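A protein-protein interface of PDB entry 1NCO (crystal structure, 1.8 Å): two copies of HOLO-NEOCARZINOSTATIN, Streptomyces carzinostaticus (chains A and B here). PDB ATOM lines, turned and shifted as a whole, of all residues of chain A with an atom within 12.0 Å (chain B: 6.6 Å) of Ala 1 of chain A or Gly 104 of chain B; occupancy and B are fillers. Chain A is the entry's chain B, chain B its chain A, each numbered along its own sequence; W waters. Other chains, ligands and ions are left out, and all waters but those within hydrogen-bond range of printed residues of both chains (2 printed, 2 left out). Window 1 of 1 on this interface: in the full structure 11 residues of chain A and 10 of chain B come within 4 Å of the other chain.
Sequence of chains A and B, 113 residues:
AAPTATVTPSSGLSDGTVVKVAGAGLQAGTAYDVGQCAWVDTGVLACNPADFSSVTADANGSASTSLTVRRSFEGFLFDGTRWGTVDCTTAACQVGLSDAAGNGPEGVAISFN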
ATOM      1  N   ALA A   1      -9.593  18.517   8.047  1.00  0.00           N
ATOM      2  CA  ALA A   1      -9.322  17.115   8.329  1.00  0.00           C
ATOM      3  C   ALA A   1      -7.824  17.211   8.289  1.00  0.00           C
ATOM      4  O   ALA A   1      -7.274  17.717   7.297  1.00  0.00           O
ATOM      5  CB  ALA A   1      -9.700  16.151   7.204  1.00  0.00           C
ATOM      6  N   ALA A   2      -7.219  16.822   9.400  1.00  0.00           N
ATOM      7  CA  ALA A   2      -5.789  16.929   9.565  1.00  0.00           C
ATOM      8  C   ALA A   2      -5.126  15.722   8.928  1.00  0.00           C
ATOM      9  O   ALA A   2      -5.744  14.642   8.823  1.00  0.00           O
ATOM     10  CB  ALA A   2      -5.477  16.999  11.055  1.00  0.00           C
ATOM     11  N   PRO A   3      -3.929  15.911   8.399  1.00  0.00           N
ATOM     12  CA  PRO A   3      -3.112  14.858   7.858  1.00  0.00           C
ATOM     13  C   PRO A   3      -2.719  13.858   8.923  1.00  0.00           C
ATOM     14  O   PRO A   3      -2.501  14.253  10.068  1.00  0.00           O
ATOM     15  CB  PRO A   3      -1.936  15.585   7.251  1.00  0.00           C
ATOM     16  CG  PRO A   3      -1.833  16.810   8.099  1.00  0.00           C
ATOM     17  CD  PRO A   3      -3.288  17.196   8.209  1.00  0.00           C
ATOM     18  N   THR A   4      -2.554  12.589   8.604  1.00  0.00           N
ATOM     19  CA  THR A   4      -2.217  11.588   9.615  1.00  0.00           C
ATOM     20  C   THR A   4      -1.000  10.784   9.155  1.00  0.00           C
ATOM     21  O   THR A   4      -0.663  10.770   7.952  1.00  0.00           O
ATOM     22  CB  THR A   4      -3.453  10.673   9.821  1.00  0.00           C
ATOM     23  OG1 THR A   4      -3.805  10.088   8.569  1.00  0.00           O
ATOM     24  CG2 THR A   4      -4.648  11.444  10.335  1.00  0.00           C
ATOM     25  N   ALA A   5      -0.308  10.109  10.081  1.00  0.00           N
ATOM     26  CA  ALA A   5       0.813   9.243   9.776  1.00  0.00           C
ATOM     27  C   ALA A   5       0.595   7.918  10.517  1.00  0.00           C
ATOM     28  O   ALA A   5      -0.005   7.944  11.599  1.00  0.00           O
ATOM     29  CB  ALA A   5       2.136   9.872  10.277  1.00  0.00           C
ATOM     30  N   GLY A  23       1.126   7.969   4.933  1.00  0.00           N
ATOM     31  CA  GLY A  23       0.617   9.292   5.198  1.00  0.00           C
ATOM     32  C   GLY A  23      -0.700   9.452   4.457  1.00  0.00           C
ATOM     33  O   GLY A  23      -0.916   8.788   3.433  1.00  0.00           O
ATOM     34  N   ALA A  24      -1.568  10.309   4.989  1.00  0.00           N
ATOM     35  CA  ALA A  24      -2.868  10.587   4.414  1.00  0.00           C
ATOM     36  C   ALA A  24      -3.172  12.038   4.752  1.00  0.00           C
ATOM     37  O   ALA A  24      -2.670  12.574   5.747  1.00  0.00           O
ATOM     38  CB  ALA A  24      -3.925   9.710   5.038  1.00  0.00           C
ATOM     39  N   GLY A  25      -3.947  12.714   3.923  1.00  0.00           N
ATOM     40  CA  GLY A  25      -4.281  14.109   4.146  1.00  0.00           C
ATOM     41  C   GLY A  25      -3.144  15.046   3.754  1.00  0.00           C
ATOM     42  O   GLY A  25      -3.088  16.216   4.163  1.00  0.00           O
ATOM     43  N   LEU A  26      -2.210  14.511   2.970  1.00  0.00           N
ATOM     44  CA  LEU A  26      -1.040  15.231   2.540  1.00  0.00           C
ATOM     45  C   LEU A  26      -1.477  15.954   1.272  1.00  0.00           C
ATOM     46  O   LEU A  26      -2.535  15.701   0.692  1.00  0.00           O
ATOM     47  CB  LEU A  26       0.109  14.244   2.234  1.00  0.00           C
ATOM     48  CG  LEU A  26       0.541  13.147   3.261  1.00  0.00           C
ATOM     49  CD1 LEU A  26       1.605  12.245   2.604  1.00  0.00           C
ATOM     50  CD2 LEU A  26       1.070  13.783   4.544  1.00  0.00           C
ATOM     51  N   GLN A  27      -0.593  16.852   0.849  1.00  0.00           N
ATOM     52  CA  GLN A  27      -0.828  17.737  -0.274  1.00  0.00           C
ATOM     53  C   GLN A  27      -0.580  17.000  -1.591  1.00  0.00           C
ATOM     54  O   GLN A  27       0.561  16.632  -1.874  1.00  0.00           O
ATOM     55  CB  GLN A  27       0.095  18.911  -0.044  1.00  0.00           C
ATOM     56  CG  GLN A  27      -0.088  19.918  -1.129  1.00  0.00           C
ATOM     57  CD  GLN A  27       0.524  21.287  -0.823  1.00  0.00           C
ATOM     58  OE1 GLN A  27       1.188  21.594   0.221  1.00  0.00           O
ATOM     59  NE2 GLN A  27       0.243  22.202  -1.772  1.00  0.00           N
ATOM     60  N   ALA A  28      -1.603  16.726  -2.415  1.00  0.00           N
ATOM     61  CA  ALA A  28      -1.433  15.933  -3.631  1.00  0.00           C
ATOM     62  C   ALA A  28      -0.326  16.469  -4.531  1.00  0.00           C
ATOM     63  O   ALA A  28      -0.201  17.676  -4.723  1.00  0.00           O
ATOM     64  CB  ALA A  28      -2.717  15.920  -4.453  1.00  0.00           C
ATOM     65  N   TYR A  32       7.669  14.590   0.096  1.00  0.00           N
ATOM     66  CA  TYR A  32       7.791  14.680   1.540  1.00  0.00           C
ATOM     67  C   TYR A  32       9.015  13.904   1.980  1.00  0.00           C
ATOM     68  O   TYR A  32       9.277  12.827   1.420  1.00  0.00           O
ATOM     69  CB  TYR A  32       6.561  14.057   2.273  1.00  0.00           C
ATOM     70  CG  TYR A  32       5.303  14.896   2.276  1.00  0.00           C
ATOM     71  CD1 TYR A  32       4.527  14.929   1.140  1.00  0.00           C
ATOM     72  CD2 TYR A  32       4.980  15.683   3.372  1.00  0.00           C
ATOM     73  CE1 TYR A  32       3.439  15.782   1.096  1.00  0.00           C
ATOM     74  CE2 TYR A  32       3.882  16.526   3.330  1.00  0.00           C
ATOM     75  CZ  TYR A  32       3.122  16.572   2.184  1.00  0.00           C
ATOM     76  OH  TYR A  32       2.040  17.420   2.066  1.00  0.00           O
ATOM     77  N   ASN A  60      -4.860  11.397  -4.157  1.00  0.00           N
ATOM     78  CA  ASN A  60      -5.698  11.410  -2.952  1.00  0.00           C
ATOM     79  C   ASN A  60      -5.032  11.976  -1.707  1.00  0.00           C
ATOM     80  O   ASN A  60      -5.684  11.986  -0.645  1.00  0.00           O
ATOM     81  CB  ASN A  60      -6.170  10.018  -2.536  1.00  0.00           C
ATOM     82  CG  ASN A  60      -7.084   9.392  -3.567  1.00  0.00           C
ATOM     83  OD1 ASN A  60      -7.943  10.097  -4.127  1.00  0.00           O
ATOM     84  ND2 ASN A  60      -6.927   8.088  -3.873  1.00  0.00           N
ATOM     85  N   GLY A  61      -3.791  12.507  -1.775  1.00  0.00           N
ATOM     86  CA  GLY A  61      -3.072  12.932  -0.585  1.00  0.00           C
ATOM     87  C   GLY A  61      -2.399  11.763   0.159  1.00  0.00           C
ATOM     88  O   GLY A  61      -1.937  11.938   1.281  1.00  0.00           O
ATOM     89  N   SER A  62      -2.299  10.548  -0.382  1.00  0.00           N
ATOM     90  CA  SER A  62      -1.719   9.430   0.320  1.00  0.00           C
ATOM     91  C   SER A  62      -0.349   8.994  -0.150  1.00  0.00           C
ATOM     92  O   SER A  62      -0.052   9.197  -1.340  1.00  0.00           O
ATOM     93  CB  SER A  62      -2.647   8.291   0.197  1.00  0.00           C
ATOM     94  OG  SER A  62      -3.819   8.638   0.908  1.00  0.00           O
ATOM     95  N   ASP A  99       7.299  18.146   4.498  1.00  0.00           N
ATOM     96  CA  ASP A  99       7.559  18.761   3.189  1.00  0.00           C
ATOM     97  C   ASP A  99       8.653  19.795   3.344  1.00  0.00           C
ATOM     98  O   ASP A  99       9.144  20.022   4.462  1.00  0.00           O
ATOM     99  CB  ASP A  99       6.319  19.465   2.621  1.00  0.00           C
ATOM    100  CG  ASP A  99       5.655  20.613   3.394  1.00  0.00           C
ATOM    101  OD1 ASP A  99       6.240  21.239   4.249  1.00  0.00           O
ATOM    102  OD2 ASP A  99       4.506  20.932   3.132  1.00  0.00           O
ATOM    103  N   ASN A 103       5.999  21.013   7.075  1.00  0.00           N
ATOM    104  CA  ASN A 103       4.615  20.662   7.263  1.00  0.00           C
ATOM    105  C   ASN A 103       4.333  19.227   6.914  1.00  0.00           C
ATOM    106  O   ASN A 103       4.935  18.605   6.012  1.00  0.00           O
ATOM    107  CB  ASN A 103       3.674  21.538   6.415  1.00  0.00           C
ATOM    108  CG  ASN A 103       3.606  22.994   6.812  1.00  0.00           C
ATOM    109  OD1 ASN A 103       4.044  23.449   7.875  1.00  0.00           O
ATOM    110  ND2 ASN A 103       3.084  23.804   5.918  1.00  0.00           N
ATOM    111  N   GLY A 104       3.336  18.720   7.636  1.00  0.00           N
ATOM    112  CA  GLY A 104       3.003  17.333   7.472  1.00  0.00           C
ATOM    113  C   GLY A 104       2.176  16.884   8.649  1.00  0.00           C
ATOM    114  O   GLY A 104       1.804  17.726   9.455  1.00  0.00           O
ATOM    115  N   PRO A 105       1.833  15.604   8.761  1.00  0.00           N
ATOM    116  CA  PRO A 105       1.142  15.017   9.918  1.00  0.00           C
ATOM    117  C   PRO A 105       1.958  15.179  11.189  1.00  0.00           C
ATOM    118  O   PRO A 105       3.160  15.447  11.182  1.00  0.00           O
ATOM    119  CB  PRO A 105       0.966  13.561   9.619  1.00  0.00           C
ATOM    120  CG  PRO A 105       1.300  13.447   8.159  1.00  0.00           C
ATOM    121  CD  PRO A 105       2.338  14.533   7.900  1.00  0.00           C
ATOM    122  N   GLU A 106       1.323  14.976  12.324  1.00  0.00           N
ATOM    123  CA  GLU A 106       2.012  14.981  13.596  1.00  0.00           C
ATOM    124  C   GLU A 106       2.948  13.774  13.645  1.00  0.00           C
ATOM    125  O   GLU A 106       2.602  12.746  13.058  1.00  0.00           O
ATOM    126  CB  GLU A 106       0.934  14.927  14.633  1.00  0.00           C
ATOM    127  CG  GLU A 106       1.502  14.938  15.993  1.00  0.00           C
ATOM    128  CD  GLU A 106       1.452  16.323  16.543  1.00  0.00           C
ATOM    129  OE1 GLU A 106       2.189  17.218  16.049  1.00  0.00           O
ATOM    130  OE2 GLU A 106       0.662  16.495  17.484  1.00  0.00           O
ATOM    131  N   PRO B   3      -0.590  20.832  11.216  1.00  0.00           N
ATOM    132  CA  PRO B   3      -1.268  22.108  11.304  1.00  0.00           C
ATOM    133  C   PRO B   3      -2.028  22.275  12.622  1.00  0.00           C
ATOM    134  O   PRO B   3      -2.648  21.317  13.107  1.00  0.00           O
ATOM    135  CB  PRO B   3      -2.185  22.140  10.109  1.00  0.00           C
ATOM    136  CG  PRO B   3      -2.533  20.675   9.927  1.00  0.00           C
ATOM    137  CD  PRO B   3      -1.238  19.945  10.280  1.00  0.00           C
ATOM    138  N   THR B   4      -2.061  23.449  13.217  1.00  0.00           N
ATOM    139  CA  THR B   4      -2.842  23.645  14.404  1.00  0.00           C
ATOM    140  C   THR B   4      -3.793  24.829  14.255  1.00  0.00           C
ATOM    141  O   THR B   4      -3.539  25.785  13.495  1.00  0.00           O
ATOM    142  CB  THR B   4      -1.891  23.864  15.572  1.00  0.00           C
ATOM    143  OG1 THR B   4      -0.980  24.878  15.161  1.00  0.00           O
ATOM    144  CG2 THR B   4      -1.193  22.610  15.993  1.00  0.00           C
ATOM    145  N   LEU B  26       0.174  25.776   8.230  1.00  0.00           N
ATOM    146  CA  LEU B  26      -0.671  25.744   7.054  1.00  0.00           C
ATOM    147  C   LEU B  26       0.194  25.869   5.802  1.00  0.00           C
ATOM    148  O   LEU B  26       1.386  26.098   5.831  1.00  0.00           O
ATOM    149  CB  LEU B  26      -1.686  26.895   7.102  1.00  0.00           C
ATOM    150  CG  LEU B  26      -2.657  27.022   8.278  1.00  0.00           C
ATOM    151  CD1 LEU B  26      -3.638  28.186   8.047  1.00  0.00           C
ATOM    152  CD2 LEU B  26      -3.398  25.704   8.433  1.00  0.00           C
ATOM    153  N   TYR B  32      -7.880  29.574   3.234  1.00  0.00           N
ATOM    154  CA  TYR B  32      -8.624  28.686   4.126  1.00  0.00           C
ATOM    155  C   TYR B  32      -9.923  29.352   4.527  1.00  0.00           C
ATOM    156  O   TYR B  32      -9.988  30.573   4.727  1.00  0.00           O
ATOM    157  CB  TYR B  32      -7.863  28.391   5.426  1.00  0.00           C
ATOM    158  CG  TYR B  32      -6.620  27.596   5.132  1.00  0.00           C
ATOM    159  CD1 TYR B  32      -5.458  28.272   4.826  1.00  0.00           C
ATOM    160  CD2 TYR B  32      -6.664  26.213   5.146  1.00  0.00           C
ATOM    161  CE1 TYR B  32      -4.316  27.562   4.520  1.00  0.00           C
ATOM    162  CE2 TYR B  32      -5.534  25.500   4.843  1.00  0.00           C
ATOM    163  CZ  TYR B  32      -4.375  26.188   4.529  1.00  0.00           C
ATOM    164  OH  TYR B  32      -3.259  25.489   4.133  1.00  0.00           O
ATOM    165  N   LEU B  97     -10.474  25.681  10.389  1.00  0.00           N
ATOM    166  CA  LEU B  97      -9.951  26.160   9.111  1.00  0.00           C
ATOM    167  C   LEU B  97      -9.825  24.982   8.155  1.00  0.00           C
ATOM    168  O   LEU B  97      -9.412  23.886   8.576  1.00  0.00           O
ATOM    169  CB  LEU B  97      -8.513  26.713   9.130  1.00  0.00           C
ATOM    170  CG  LEU B  97      -7.749  27.789   9.928  1.00  0.00           C
ATOM    171  CD1 LEU B  97      -8.464  29.084   9.854  1.00  0.00           C
ATOM    172  CD2 LEU B  97      -7.592  27.363  11.374  1.00  0.00           C
ATOM    173  N   SER B  98     -10.164  25.145   6.865  1.00  0.00           N
ATOM    174  CA  SER B  98      -9.902  24.105   5.859  1.00  0.00           C
ATOM    175  C   SER B  98      -9.739  24.754   4.490  1.00  0.00           C
ATOM    176  O   SER B  98     -10.247  25.861   4.279  1.00  0.00           O
ATOM    177  CB  SER B  98     -11.032  23.091   5.802  1.00  0.00           C
ATOM    178  OG  SER B  98     -12.253  23.803   5.745  1.00  0.00           O
ATOM    179  N   ASP B  99      -8.949  24.145   3.615  1.00  0.00           N
ATOM    180  CA  ASP B  99      -8.718  24.705   2.282  1.00  0.00           C
ATOM    181  C   ASP B  99      -9.696  24.111   1.281  1.00  0.00           C
ATOM    182  O   ASP B  99     -10.598  23.377   1.709  1.00  0.00           O
ATOM    183  CB  ASP B  99      -7.271  24.419   1.869  1.00  0.00           C
ATOM    184  CG  ASP B  99      -6.824  22.969   1.670  1.00  0.00           C
ATOM    185  OD1 ASP B  99      -7.636  22.038   1.664  1.00  0.00           O
ATOM    186  OD2 ASP B  99      -5.630  22.749   1.501  1.00  0.00           O
ATOM    187  N   GLY B 102     -10.247  20.410   1.623  1.00  0.00           N
ATOM    188  CA  GLY B 102     -10.840  19.871   2.874  1.00  0.00           C
ATOM    189  C   GLY B 102      -9.772  19.473   3.886  1.00  0.00           C
ATOM    190  O   GLY B 102      -9.983  18.824   4.939  1.00  0.00           O
ATOM    191  N   ASN B 103      -8.579  19.943   3.595  1.00  0.00           N
ATOM    192  CA  ASN B 103      -7.427  19.632   4.385  1.00  0.00           C
ATOM    193  C   ASN B 103      -7.146  20.772   5.334  1.00  0.00           C
ATOM    194  O   ASN B 103      -7.316  21.962   5.007  1.00  0.00           O
ATOM    195  CB  ASN B 103      -6.238  19.396   3.457  1.00  0.00           C
ATOM    196  CG  ASN B 103      -6.258  18.050   2.759  1.00  0.00           C
ATOM    197  OD1 ASN B 103      -7.310  17.439   2.551  1.00  0.00           O
ATOM    198  ND2 ASN B 103      -5.124  17.517   2.350  1.00  0.00           N
ATOM    199  N   GLY B 104      -6.702  20.431   6.535  1.00  0.00           N
ATOM    200  CA  GLY B 104      -6.406  21.498   7.482  1.00  0.00           C
ATOM    201  C   GLY B 104      -6.278  20.968   8.893  1.00  0.00           C
ATOM    202  O   GLY B 104      -6.338  19.752   9.084  1.00  0.00           O
ATOM    203  N   PRO B 105      -6.150  21.853   9.887  1.00  0.00           N
ATOM    204  CA  PRO B 105      -6.037  21.490  11.296  1.00  0.00           C
ATOM    205  C   PRO B 105      -7.312  20.810  11.790  1.00  0.00           C
ATOM    206  O   PRO B 105      -8.410  20.972  11.228  1.00  0.00           O
ATOM    207  CB  PRO B 105      -5.786  22.795  12.025  1.00  0.00           C
ATOM    208  CG  PRO B 105      -5.515  23.794  10.907  1.00  0.00           C
ATOM    209  CD  PRO B 105      -6.334  23.292   9.742  1.00  0.00           C
ATOM    210  N   GLU B 106      -7.212  20.019  12.844  1.00  0.00           N
ATOM    211  CA  GLU B 106      -8.425  19.557  13.483  1.00  0.00           C
ATOM    212  C   GLU B 106      -9.177  20.766  14.068  1.00  0.00           C
ATOM    213  O   GLU B 106      -8.547  21.776  14.416  1.00  0.00           O
ATOM    214  CB  GLU B 106      -8.044  18.592  14.554  1.00  0.00           C
ATOM    215  CG  GLU B 106      -7.911  17.149  14.015  1.00  0.00           C
ATOM    216  CD  GLU B 106      -7.234  16.260  15.075  1.00  0.00           C
ATOM    217  OE1 GLU B 106      -7.488  16.481  16.282  1.00  0.00           O
ATOM    218  OE2 GLU B 106      -6.422  15.370  14.707  1.00  0.00           O
ATOM    219  N   GLY B 107     -10.508  20.733  14.110  1.00  0.00           N
ATOM    220  CA  GLY B 107     -11.305  21.810  14.677  1.00  0.00           C
ATOM    221  C   GLY B 107     -11.109  21.942  16.185  1.00  0.00           C
ATOM    222  O   GLY B 107     -10.522  21.060  16.805  1.00  0.00           O
HETATM  223  O   HOH W   1      -4.719  18.109   5.742  1.00  0.00           O
HETATM  224  O   HOH W   2      -5.563  14.941   1.131  1.00  0.00           O
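Water W2 lies within hydrogen-bond range of the side-chain amide nitrogen of Asn 103 of chain B, the backbone carbonyl oxygen of Leu 26 of chain A and the backbone carbonyl oxygen of Asn 60 of chain A.
Water W1 lies within hydrogen-bond range of the backbone carbonyl oxygen of Gly 25 of chain A (3.0 Å), the backbone carbonyl oxygen of Ala 1 of chain A (3.0 Å), the backbone NH of Gly 104 of chain B (3.2 Å) and the side-chain amide nitrogen of Asn 103 of chain B (3.5 Å).
Of the printed residues of chain B, Ala 2 of chain A touches Gly 104 (2.9 Å) and Glu 106 (3.8 Å).
Of the printed residues of chain B, Gly 25 of chain A touches Asn 103 (3.0 Å).
Of the printed residues of chain B, Asn 103 of chain A touches Leu 26.
Pro 3 of chain B touches two residues of chain A.
Of the printed residues of chain A, Leu 26 of chain B touches Asn 103 (2.9 Å).
Tyr 32 of chain B touches none of the printed residues of chain A.
No residue of chain A comes within 4 Å of Ser 98 of chain B.
Gly 102 of chain B touches just one residue of chain A: Ala 1.
Asn 103 of chain B touches three residues of chain A.
Gly 104 of chain B touches two residues of chain A.
No residue of chain A comes within 4 Å of Pro 105 of chain B.
The nearest printed residue of chain A that does not touch Leu 26 of chain B is Asp 99 of chain A (6.6 Å).
Pro 3 of chain B touches its own counterpart, Pro 3 of chain A.
Leu 26 of chain A touches Asn 103 of chain B, and with the chains exchanged Asn 103 of chain A touches Leu 26 of chain B.
Gly 104 of chain A touches Pro 3 of chain B, but with the chains exchanged Pro 3 of chain A does not touch Gly 104 of chain B (4.1 Å).
Of the 10 pairs that touch across the chains among the printed residues, 3 have their exchanged pair printed and touching as well.
Among the printed residues, merely in contact across the chains: Ala 1 of chain A with Asn 103 of chain B, Leu 26 of chain A with Asn 103 of chain B, Ala 2 of chain A with Glu 106 of chain B, Gly 104 of chain A with Pro 3 of chain B and Pro 3 of chain A with Pro 3 of chain B.
Of the 13 printed residues of chain B, 6 touch a printed residue of chain A.
Hydrophobic or aromatic side chains of chain B within 4 Å of the printed part of chain A: Pro 3.
Along chain B the printed residues that touch a printed residue of chain A span positions 3 to 106.
Among the printed residues, no Asp or Glu carboxylate lies within 4 Å of a Lys or Arg side-chain nitrogen of the other chain.
The backbone NH of Gly 25 of chain A sits at hydrogen-bond distance from the backbone carbonyl oxygen of Gly 61 of chain A, 3.4 Å away.
N of Asn 103 of chain A sits at hydrogen-bond distance from OD1 of Asp 99 of chain A (2.8 Å).
The backbone NH of Leu 26 of chain A is in hydrogen-bond range of the backbone carbonyl oxygen of Gly 61 of chain A.
OD1 of Asp 99 of chain B sits at hydrogen-bond distance from N of Gly 102 of chain B.
The backbone NH (N) of Asn 103 of chain B sits at hydrogen-bond distance from the side-chain carboxylate (OD1) of Asp 99 of chain B.
ND2 of Asn 103 of chain A lies within hydrogen-bond range of O of Leu 26 of chain B, 2.9 Å away.
O of Gly 102 of chain B sits at hydrogen-bond distance from N of Ala 1 of chain A, at 3.1 Å.
The backbone NH (N) of Ala 2 of chain A sits close to the backbone carbonyl oxygen (O) of Gly 104 of chain B, at 3.1 Å.
ND2 of Asn 103 of chain B sits at hydrogen-bond distance from O of Gly 25 of chain A (3.0 Å).
The backbone NH of Gly 104 of chain B is in hydrogen-bond range of the backbone carbonyl oxygen of Ala 1 of chain A, at 2.9 Å.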
